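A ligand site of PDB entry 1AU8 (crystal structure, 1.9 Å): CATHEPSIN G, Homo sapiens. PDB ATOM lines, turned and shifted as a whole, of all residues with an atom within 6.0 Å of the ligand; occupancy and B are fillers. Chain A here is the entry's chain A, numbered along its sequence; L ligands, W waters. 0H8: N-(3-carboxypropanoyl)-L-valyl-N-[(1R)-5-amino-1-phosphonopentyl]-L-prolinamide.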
ATOM      1  N   ARG A  28      -1.521  -8.344  17.097  1.00  0.00           N
ATOM      2  CA  ARG A  28      -2.243  -8.602  18.371  1.00  0.00           C
ATOM      3  C   ARG A  28      -3.055  -9.900  18.302  1.00  0.00           C
ATOM      4  O   ARG A  28      -3.493 -10.339  17.225  1.00  0.00           O
ATOM      5  CB  ARG A  28      -3.187  -7.448  18.697  1.00  0.00           C
ATOM      6  CG  ARG A  28      -4.368  -7.335  17.733  1.00  0.00           C
ATOM      7  CD  ARG A  28      -4.005  -6.683  16.397  1.00  0.00           C
ATOM      8  NE  ARG A  28      -5.162  -6.433  15.538  1.00  0.00           N
ATOM      9  CZ  ARG A  28      -5.693  -7.348  14.713  1.00  0.00           C
ATOM     10  NH1 ARG A  28      -5.192  -8.592  14.639  1.00  0.00           N
ATOM     11  NH2 ARG A  28      -6.752  -7.130  13.924  1.00  0.00           N
ATOM     12  N   CYS A  29      -3.172 -10.535  19.502  1.00  0.00           N
ATOM     13  CA  CYS A  29      -3.905 -11.787  19.666  1.00  0.00           C
ATOM     14  C   CYS A  29      -4.522 -11.849  21.040  1.00  0.00           C
ATOM     15  O   CYS A  29      -4.348 -10.960  21.856  1.00  0.00           O
ATOM     16  CB  CYS A  29      -2.961 -12.973  19.531  1.00  0.00           C
ATOM     17  SG  CYS A  29      -2.560 -13.478  17.841  1.00  0.00           S
ATOM     18  N   HIS A  44       0.392 -19.476  15.913  1.00  0.00           N
ATOM     19  CA  HIS A  44       0.549 -18.536  14.808  1.00  0.00           C
ATOM     20  C   HIS A  44       0.692 -17.111  15.317  1.00  0.00           C
ATOM     21  O   HIS A  44       1.095 -16.230  14.584  1.00  0.00           O
ATOM     22  CB  HIS A  44      -0.540 -18.728  13.715  1.00  0.00           C
ATOM     23  CG  HIS A  44      -1.833 -17.994  13.965  1.00  0.00           C
ATOM     24  ND1 HIS A  44      -2.976 -18.631  14.396  1.00  0.00           N
ATOM     25  CD2 HIS A  44      -2.181 -16.696  13.764  1.00  0.00           C
ATOM     26  CE1 HIS A  44      -3.970 -17.769  14.442  1.00  0.00           C
ATOM     27  NE2 HIS A  44      -3.517 -16.593  14.076  1.00  0.00           N
ATOM     28  N   CYS A  45       0.425 -16.915  16.602  1.00  0.00           N
ATOM     29  CA  CYS A  45       0.559 -15.613  17.260  1.00  0.00           C
ATOM     30  C   CYS A  45       1.978 -15.432  17.804  1.00  0.00           C
ATOM     31  O   CYS A  45       2.241 -14.484  18.539  1.00  0.00           O
ATOM     32  CB  CYS A  45      -0.402 -15.504  18.446  1.00  0.00           C
ATOM     33  SG  CYS A  45      -2.150 -15.453  18.004  1.00  0.00           S
ATOM     34  N   ILE A  85      -1.676 -24.765   9.011  1.00  0.00           N
ATOM     35  CA  ILE A  85      -2.168 -24.167  10.274  1.00  0.00           C
ATOM     36  C   ILE A  85      -2.675 -25.257  11.224  1.00  0.00           C
ATOM     37  O   ILE A  85      -3.718 -25.114  11.867  1.00  0.00           O
ATOM     38  CB  ILE A  85      -3.320 -23.196  10.004  1.00  0.00           C
ATOM     39  CG1 ILE A  85      -3.056 -22.292   8.796  1.00  0.00           C
ATOM     40  CG2 ILE A  85      -3.578 -22.247  11.179  1.00  0.00           C
ATOM     41  CD1 ILE A  85      -4.237 -21.360   8.480  1.00  0.00           C
ATOM     42  N   ASP A  88      -1.989 -25.631  15.991  1.00  0.00           N
ATOM     43  CA  ASP A  88      -1.924 -24.186  16.296  1.00  0.00           C
ATOM     44  C   ASP A  88      -2.187 -23.933  17.780  1.00  0.00           C
ATOM     45  O   ASP A  88      -3.287 -23.496  18.176  1.00  0.00           O
ATOM     46  CB  ASP A  88      -2.982 -23.453  15.471  1.00  0.00           C
ATOM     47  CG  ASP A  88      -2.731 -21.960  15.357  1.00  0.00           C
ATOM     48  OD1 ASP A  88      -1.623 -21.454  15.780  1.00  0.00           O
ATOM     49  OD2 ASP A  88      -3.636 -21.197  14.845  1.00  0.00           O
ATOM     50  N   ILE A 155     -14.895 -28.625   3.782  1.00  0.00           N
ATOM     51  CA  ILE A 155     -14.651 -27.204   3.485  1.00  0.00           C
ATOM     52  C   ILE A 155     -13.157 -26.839   3.584  1.00  0.00           C
ATOM     53  O   ILE A 155     -12.655 -26.005   2.828  1.00  0.00           O
ATOM     54  CB  ILE A 155     -15.430 -26.300   4.476  1.00  0.00           C
ATOM     55  CG1 ILE A 155     -16.859 -26.825   4.659  1.00  0.00           C
ATOM     56  CG2 ILE A 155     -15.436 -24.872   3.972  1.00  0.00           C
ATOM     57  CD1 ILE A 155     -17.550 -26.298   5.904  1.00  0.00           C
ATOM     58  N   PHE A 156     -12.489 -27.410   4.569  1.00  0.00           N
ATOM     59  CA  PHE A 156     -11.075 -27.145   4.812  1.00  0.00           C
ATOM     60  C   PHE A 156     -10.266 -28.414   4.557  1.00  0.00           C
ATOM     61  O   PHE A 156     -10.506 -29.445   5.181  1.00  0.00           O
ATOM     62  CB  PHE A 156     -10.873 -26.649   6.241  1.00  0.00           C
ATOM     63  CG  PHE A 156     -11.625 -25.390   6.558  1.00  0.00           C
ATOM     64  CD1 PHE A 156     -11.256 -24.189   5.973  1.00  0.00           C
ATOM     65  CD2 PHE A 156     -12.713 -25.413   7.425  1.00  0.00           C
ATOM     66  CE1 PHE A 156     -11.961 -23.040   6.236  1.00  0.00           C
ATOM     67  CE2 PHE A 156     -13.420 -24.260   7.698  1.00  0.00           C
ATOM     68  CZ  PHE A 156     -13.050 -23.082   7.110  1.00  0.00           C
ATOM     69  N   ALA A 175     -19.129 -15.053  14.639  1.00  0.00           N
ATOM     70  CA  ALA A 175     -17.829 -15.707  14.481  1.00  0.00           C
ATOM     71  C   ALA A 175     -16.711 -14.907  15.129  1.00  0.00           C
ATOM     72  O   ALA A 175     -16.903 -13.756  15.527  1.00  0.00           O
ATOM     73  CB  ALA A 175     -17.526 -15.859  12.987  1.00  0.00           C
ATOM     74  N   ALA A 176     -15.553 -15.560  15.279  1.00  0.00           N
ATOM     75  CA  ALA A 176     -14.395 -14.861  15.813  1.00  0.00           C
ATOM     76  C   ALA A 176     -13.858 -14.174  14.561  1.00  0.00           C
ATOM     77  O   ALA A 176     -14.240 -14.532  13.452  1.00  0.00           O
ATOM     78  CB  ALA A 176     -13.394 -15.850  16.342  1.00  0.00           C
ATOM     79  N   PHE A 177     -12.997 -13.182  14.734  1.00  0.00           N
ATOM     80  CA  PHE A 177     -12.456 -12.450  13.597  1.00  0.00           C
ATOM     81  C   PHE A 177     -11.014 -12.055  13.870  1.00  0.00           C
ATOM     82  O   PHE A 177     -10.403 -12.528  14.823  1.00  0.00           O
ATOM     83  CB  PHE A 177     -13.334 -11.234  13.303  1.00  0.00           C
ATOM     84  CG  PHE A 177     -13.282 -10.784  11.876  1.00  0.00           C
ATOM     85  CD1 PHE A 177     -13.251 -11.718  10.840  1.00  0.00           C
ATOM     86  CD2 PHE A 177     -13.217  -9.434  11.566  1.00  0.00           C
ATOM     87  CE1 PHE A 177     -13.137 -11.298   9.507  1.00  0.00           C
ATOM     88  CE2 PHE A 177     -13.098  -8.997  10.249  1.00  0.00           C
ATOM     89  CZ  PHE A 177     -13.056  -9.922   9.212  1.00  0.00           C
ATOM     90  N   LYS A 178     -10.480 -11.146  13.146  1.00  0.00           N
ATOM     91  CA  LYS A 178      -9.068 -10.751  13.146  1.00  0.00           C
ATOM     92  C   LYS A 178      -8.723 -10.051  14.458  1.00  0.00           C
ATOM     93  O   LYS A 178      -9.407  -9.115  14.892  1.00  0.00           O
ATOM     94  CB  LYS A 178      -8.801  -9.804  11.964  1.00  0.00           C
ATOM     95  CG  LYS A 178      -8.995 -10.495  10.617  1.00  0.00           C
ATOM     96  CD  LYS A 178      -8.774  -9.576   9.414  1.00  0.00           C
ATOM     97  CE  LYS A 178      -8.683 -10.347   8.092  1.00  0.00           C
ATOM     98  NZ  LYS A 178      -9.688 -11.414   7.981  1.00  0.00           N
ATOM     99  N   GLY A 179      -7.794 -10.765  15.177  1.00  0.00           N
ATOM    100  CA  GLY A 179      -7.411 -10.282  16.489  1.00  0.00           C
ATOM    101  C   GLY A 179      -7.921 -11.146  17.600  1.00  0.00           C
ATOM    102  O   GLY A 179      -7.474 -11.021  18.732  1.00  0.00           O
ATOM    103  N   ASP A 180      -8.859 -12.043  17.302  1.00  0.00           N
ATOM    104  CA  ASP A 180      -9.419 -12.930  18.321  1.00  0.00           C
ATOM    105  C   ASP A 180      -8.655 -14.216  18.450  1.00  0.00           C
ATOM    106  O   ASP A 180      -8.910 -14.987  19.373  1.00  0.00           O
ATOM    107  CB  ASP A 180     -10.894 -13.259  18.046  1.00  0.00           C
ATOM    108  CG  ASP A 180     -11.808 -12.054  18.180  1.00  0.00           C
ATOM    109  OD1 ASP A 180     -11.720 -11.335  19.179  1.00  0.00           O
ATOM    110  OD2 ASP A 180     -12.628 -11.815  17.285  1.00  0.00           O
ATOM    111  N   SER A 181      -7.730 -14.463  17.533  1.00  0.00           N
ATOM    112  CA  SER A 181      -6.913 -15.667  17.552  1.00  0.00           C
ATOM    113  C   SER A 181      -6.264 -15.913  18.887  1.00  0.00           C
ATOM    114  O   SER A 181      -5.753 -14.973  19.475  1.00  0.00           O
ATOM    115  CB  SER A 181      -5.823 -15.594  16.488  1.00  0.00           C
ATOM    116  OG  SER A 181      -6.319 -15.940  15.203  1.00  0.00           O
ATOM    117  N   GLY A 182      -6.310 -17.153  19.367  1.00  0.00           N
ATOM    118  CA  GLY A 182      -5.639 -17.519  20.623  1.00  0.00           C
ATOM    119  C   GLY A 182      -6.626 -17.487  21.802  1.00  0.00           C
ATOM    120  O   GLY A 182      -6.321 -18.007  22.889  1.00  0.00           O
ATOM    121  N   VAL A 195      -9.140 -20.149  19.270  1.00  0.00           N
ATOM    122  CA  VAL A 195      -9.418 -19.535  17.962  1.00  0.00           C
ATOM    123  C   VAL A 195      -8.187 -19.698  17.084  1.00  0.00           C
ATOM    124  O   VAL A 195      -7.070 -19.351  17.488  1.00  0.00           O
ATOM    125  CB  VAL A 195      -9.737 -18.061  18.151  1.00  0.00           C
ATOM    126  CG1 VAL A 195      -9.931 -17.333  16.816  1.00  0.00           C
ATOM    127  CG2 VAL A 195     -11.034 -17.852  18.949  1.00  0.00           C
ATOM    128  N   SER A 196      -8.402 -20.216  15.894  1.00  0.00           N
ATOM    129  CA  SER A 196      -7.291 -20.466  14.969  1.00  0.00           C
ATOM    130  C   SER A 196      -7.514 -19.818  13.593  1.00  0.00           C
ATOM    131  O   SER A 196      -6.853 -18.830  13.244  1.00  0.00           O
ATOM    132  CB  SER A 196      -7.087 -21.970  14.798  1.00  0.00           C
ATOM    133  OG  SER A 196      -5.926 -22.209  14.013  1.00  0.00           O
ATOM    134  N   TYR A 197      -8.427 -20.353  12.774  1.00  0.00           N
ATOM    135  CA  TYR A 197      -8.644 -19.769  11.426  1.00  0.00           C
ATOM    136  C   TYR A 197     -10.016 -20.124  10.832  1.00  0.00           C
ATOM    137  O   TYR A 197     -10.768 -20.942  11.377  1.00  0.00           O
ATOM    138  CB  TYR A 197      -7.537 -20.259  10.466  1.00  0.00           C
ATOM    139  CG  TYR A 197      -7.683 -21.725  10.017  1.00  0.00           C
ATOM    140  CD1 TYR A 197      -7.217 -22.761  10.836  1.00  0.00           C
ATOM    141  CD2 TYR A 197      -8.276 -22.022   8.788  1.00  0.00           C
ATOM    142  CE1 TYR A 197      -7.343 -24.098  10.416  1.00  0.00           C
ATOM    143  CE2 TYR A 197      -8.413 -23.355   8.376  1.00  0.00           C
ATOM    144  CZ  TYR A 197      -7.946 -24.395   9.185  1.00  0.00           C
ATOM    145  OH  TYR A 197      -8.066 -25.683   8.780  1.00  0.00           O
ATOM    146  N   GLY A 198     -10.298 -19.475   9.719  1.00  0.00           N
ATOM    147  CA  GLY A 198     -11.561 -19.656   8.979  1.00  0.00           C
ATOM    148  C   GLY A 198     -11.477 -18.923   7.642  1.00  0.00           C
ATOM    149  O   GLY A 198     -10.388 -18.501   7.209  1.00  0.00           O
ATOM    150  N   LYS A 199     -12.620 -18.769   7.003  1.00  0.00           N
ATOM    151  CA  LYS A 199     -12.702 -18.049   5.720  1.00  0.00           C
ATOM    152  C   LYS A 199     -12.325 -16.593   5.963  1.00  0.00           C
ATOM    153  O   LYS A 199     -12.764 -15.980   6.945  1.00  0.00           O
ATOM    154  CB  LYS A 199     -14.117 -18.096   5.133  1.00  0.00           C
ATOM    155  CG  LYS A 199     -14.569 -19.490   4.714  1.00  0.00           C
ATOM    156  CD  LYS A 199     -15.975 -19.489   4.086  1.00  0.00           C
ATOM    157  CE  LYS A 199     -16.575 -20.888   3.955  1.00  0.00           C
ATOM    158  NZ  LYS A 199     -17.247 -21.342   5.178  1.00  0.00           N
ATOM    159  N   SER A 200     -11.670 -15.915   5.053  1.00  0.00           N
ATOM    160  CA  SER A 200     -11.351 -14.495   5.196  1.00  0.00           C
ATOM    161  C   SER A 200     -12.601 -13.654   5.422  1.00  0.00           C
ATOM    162  O   SER A 200     -12.563 -12.623   6.091  1.00  0.00           O
ATOM    163  CB  SER A 200     -10.612 -13.991   3.946  1.00  0.00           C
ATOM    164  OG  SER A 200     -11.460 -14.033   2.805  1.00  0.00           O
ATOM    165  N   SER A 201     -13.723 -14.103   4.872  1.00  0.00           N
ATOM    166  CA  SER A 201     -14.993 -13.394   4.981  1.00  0.00           C
ATOM    167  C   SER A 201     -15.493 -13.323   6.406  1.00  0.00           C
ATOM    168  O   SER A 201     -16.177 -12.375   6.791  1.00  0.00           O
ATOM    169  CB  SER A 201     -16.054 -14.081   4.112  1.00  0.00           C
ATOM    170  OG  SER A 201     -16.259 -15.419   4.539  1.00  0.00           O
ATOM    171  N   GLY A 202     -15.161 -14.349   7.177  1.00  0.00           N
ATOM    172  CA  GLY A 202     -15.616 -14.408   8.556  1.00  0.00           C
ATOM    173  C   GLY A 202     -16.884 -15.246   8.574  1.00  0.00           C
ATOM    174  O   GLY A 202     -17.505 -15.438   9.624  1.00  0.00           O
ATOM    175  N   GLU A 206     -15.945 -22.010  11.291  1.00  0.00           N
ATOM    176  CA  GLU A 206     -14.495 -21.817  11.384  1.00  0.00           C
ATOM    177  C   GLU A 206     -13.858 -22.947  12.183  1.00  0.00           C
ATOM    178  O   GLU A 206     -14.535 -23.895  12.600  1.00  0.00           O
ATOM    179  CB  GLU A 206     -14.187 -20.496  12.087  1.00  0.00           C
ATOM    180  CG  GLU A 206     -14.897 -20.350  13.429  1.00  0.00           C
ATOM    181  CD  GLU A 206     -14.752 -18.954  14.028  1.00  0.00           C
ATOM    182  OE1 GLU A 206     -13.621 -18.337  13.924  1.00  0.00           O
ATOM    183  OE2 GLU A 206     -15.748 -18.400  14.623  1.00  0.00           O
HETATM  184  C1  0H8 L   1     -10.143 -19.924   3.499  1.00  0.00           C
HETATM  185  O1  0H8 L   1     -10.972 -19.214   2.839  1.00  0.00           O
HETATM  186  O2  0H8 L   1     -10.120 -21.351   3.386  1.00  0.00           O
HETATM  187  C2  0H8 L   1      -8.976 -19.195   4.167  1.00  0.00           C
HETATM  188  C3  0H8 L   1      -8.465 -19.941   5.419  1.00  0.00           C
HETATM  189  C4  0H8 L   1      -7.374 -19.148   6.097  1.00  0.00           C
HETATM  190  O4  0H8 L   1      -6.203 -19.528   6.016  1.00  0.00           O
HETATM  191  N   0H8 L   1      -7.711 -17.911   6.446  1.00  0.00           N
HETATM  192  CA  0H8 L   1      -6.716 -16.959   6.891  1.00  0.00           C
HETATM  193  C   0H8 L   1      -6.619 -16.991   8.413  1.00  0.00           C
HETATM  194  O   0H8 L   1      -7.523 -17.493   9.080  1.00  0.00           O
HETATM  195  CB  0H8 L   1      -7.040 -15.516   6.382  1.00  0.00           C
HETATM  196  CG1 0H8 L   1      -8.286 -14.975   7.044  1.00  0.00           C
HETATM  197  CG2 0H8 L   1      -5.868 -14.595   6.638  1.00  0.00           C
HETATM  198  N1  0H8 L   1      -5.652 -17.371   9.270  1.00  0.00           N
HETATM  199  CA1 0H8 L   1      -5.536 -17.277  10.734  1.00  0.00           C
HETATM  200  C5  0H8 L   1      -6.136 -15.987  11.286  1.00  0.00           C
HETATM  201  O3  0H8 L   1      -6.042 -14.946  10.667  1.00  0.00           O
HETATM  202  CB1 0H8 L   1      -4.025 -17.388  10.967  1.00  0.00           C
HETATM  203  CG  0H8 L   1      -3.423 -16.883   9.728  1.00  0.00           C
HETATM  204  CD  0H8 L   1      -4.308 -17.457   8.654  1.00  0.00           C
HETATM  205  N2  0H8 L   1      -6.813 -16.085  12.427  1.00  0.00           N
HETATM  206  CA2 0H8 L   1      -7.224 -15.206  12.840  1.00  0.00           C
HETATM  207  P   0H8 L   1      -6.308 -14.633  14.321  1.00  0.00           P
HETATM  208  O1P 0H8 L   1      -4.919 -14.192  13.786  1.00  0.00           O
HETATM  209  O2P 0H8 L   1      -6.777 -13.210  14.816  1.00  0.00           O
HETATM  210  CB2 0H8 L   1      -8.653 -15.422  13.339  1.00  0.00           C
HETATM  211  CG3 0H8 L   1      -9.562 -15.641  12.179  1.00  0.00           C
HETATM  212  CD1 0H8 L   1     -10.980 -15.951  12.686  1.00  0.00           C
HETATM  213  CE  0H8 L   1     -11.809 -16.255  11.458  1.00  0.00           C
HETATM  214  NZ  0H8 L   1     -13.138 -16.684  11.815  1.00  0.00           N
HETATM  215  O   HOH W   1     -14.052 -17.142   9.222  1.00  0.00           O
HETATM  216  O   HOH W   2      -2.785 -13.113  11.770  1.00  0.00           O
HETATM  217  O   HOH W   3      -6.100 -11.641  10.560  1.00  0.00           O
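Water W1 bridges a nitrogen (NZ) of the ligand and the backbone carbonyl oxygen of Lys 199.
N of the ligand lies within hydrogen-bond range of O of Gly 198 (2.8 Å). The side-chain hydroxyl (OG) of Ser 181 is bonded to a phosphorus (P) of the ligand (1.6 Å). The side-chain carboxylate (OE1) of Glu 206 lies within salt-bridge range of a nitrogen (NZ) of the ligand. An oxygen (O2P) of the ligand is in hydrogen-bond range of the backbone NH (N) of Asp 180, at 3.4 Å. The backbone NH (N) of Gly 179 is in hydrogen-bond range of an oxygen (O2P) of the ligand. A ring nitrogen (NE2) of His 44 sits at hydrogen-bond distance from an oxygen (O1P) of the ligand (2.8 Å). N of Gly 198 is in hydrogen-bond range of O of the ligand (3.5 Å). The backbone carbonyl oxygen (O) of Ser 196 is in hydrogen-bond range of a nitrogen (N2) of the ligand, at 2.9 Å. The backbone NH of Ser 181 sits close to an oxygen (O2P) of the ligand (3.1 Å). NZ of the ligand is in hydrogen-bond range of O of Ala 176, at 2.9 Å.
Residues that only touch the ligand: Ile 85, Phe 156, Phe 177, Lys 178, Tyr 197, Lys 199 and Ser 200. Hydrophobic or aromatic side chains that line the ligand: His 44, Ile 85, Phe 156 and Tyr 197. Along chain A the residues within 4 Å of the ligand span positions 44 to 206.
OG of Ser 181 sits close to NE2 of His 44, 3.1 Å away. The side-chain carboxylate (OD2) of Asp 88 lies within hydrogen-bond range of a ring nitrogen (ND1) of His 44, 2.7 Å away. OD2 of Asp 88 lies within hydrogen-bond range of OG of Ser 196, at 2.6 Å. The backbone NH (N) of Ala 176 is in hydrogen-bond range of the side-chain carboxylate (OE2) of Glu 206 (2.9 Å). SG of Cys 45 forms a disulfide with SG of Cys 29 (2.0 Å). The guanidinium group (NH2) of Arg 28 is in hydrogen-bond range of the backbone carbonyl oxygen (O) of Lys 178. N of Phe 177 is in hydrogen-bond range of OD2 of Asp 180 (2.9 Å).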
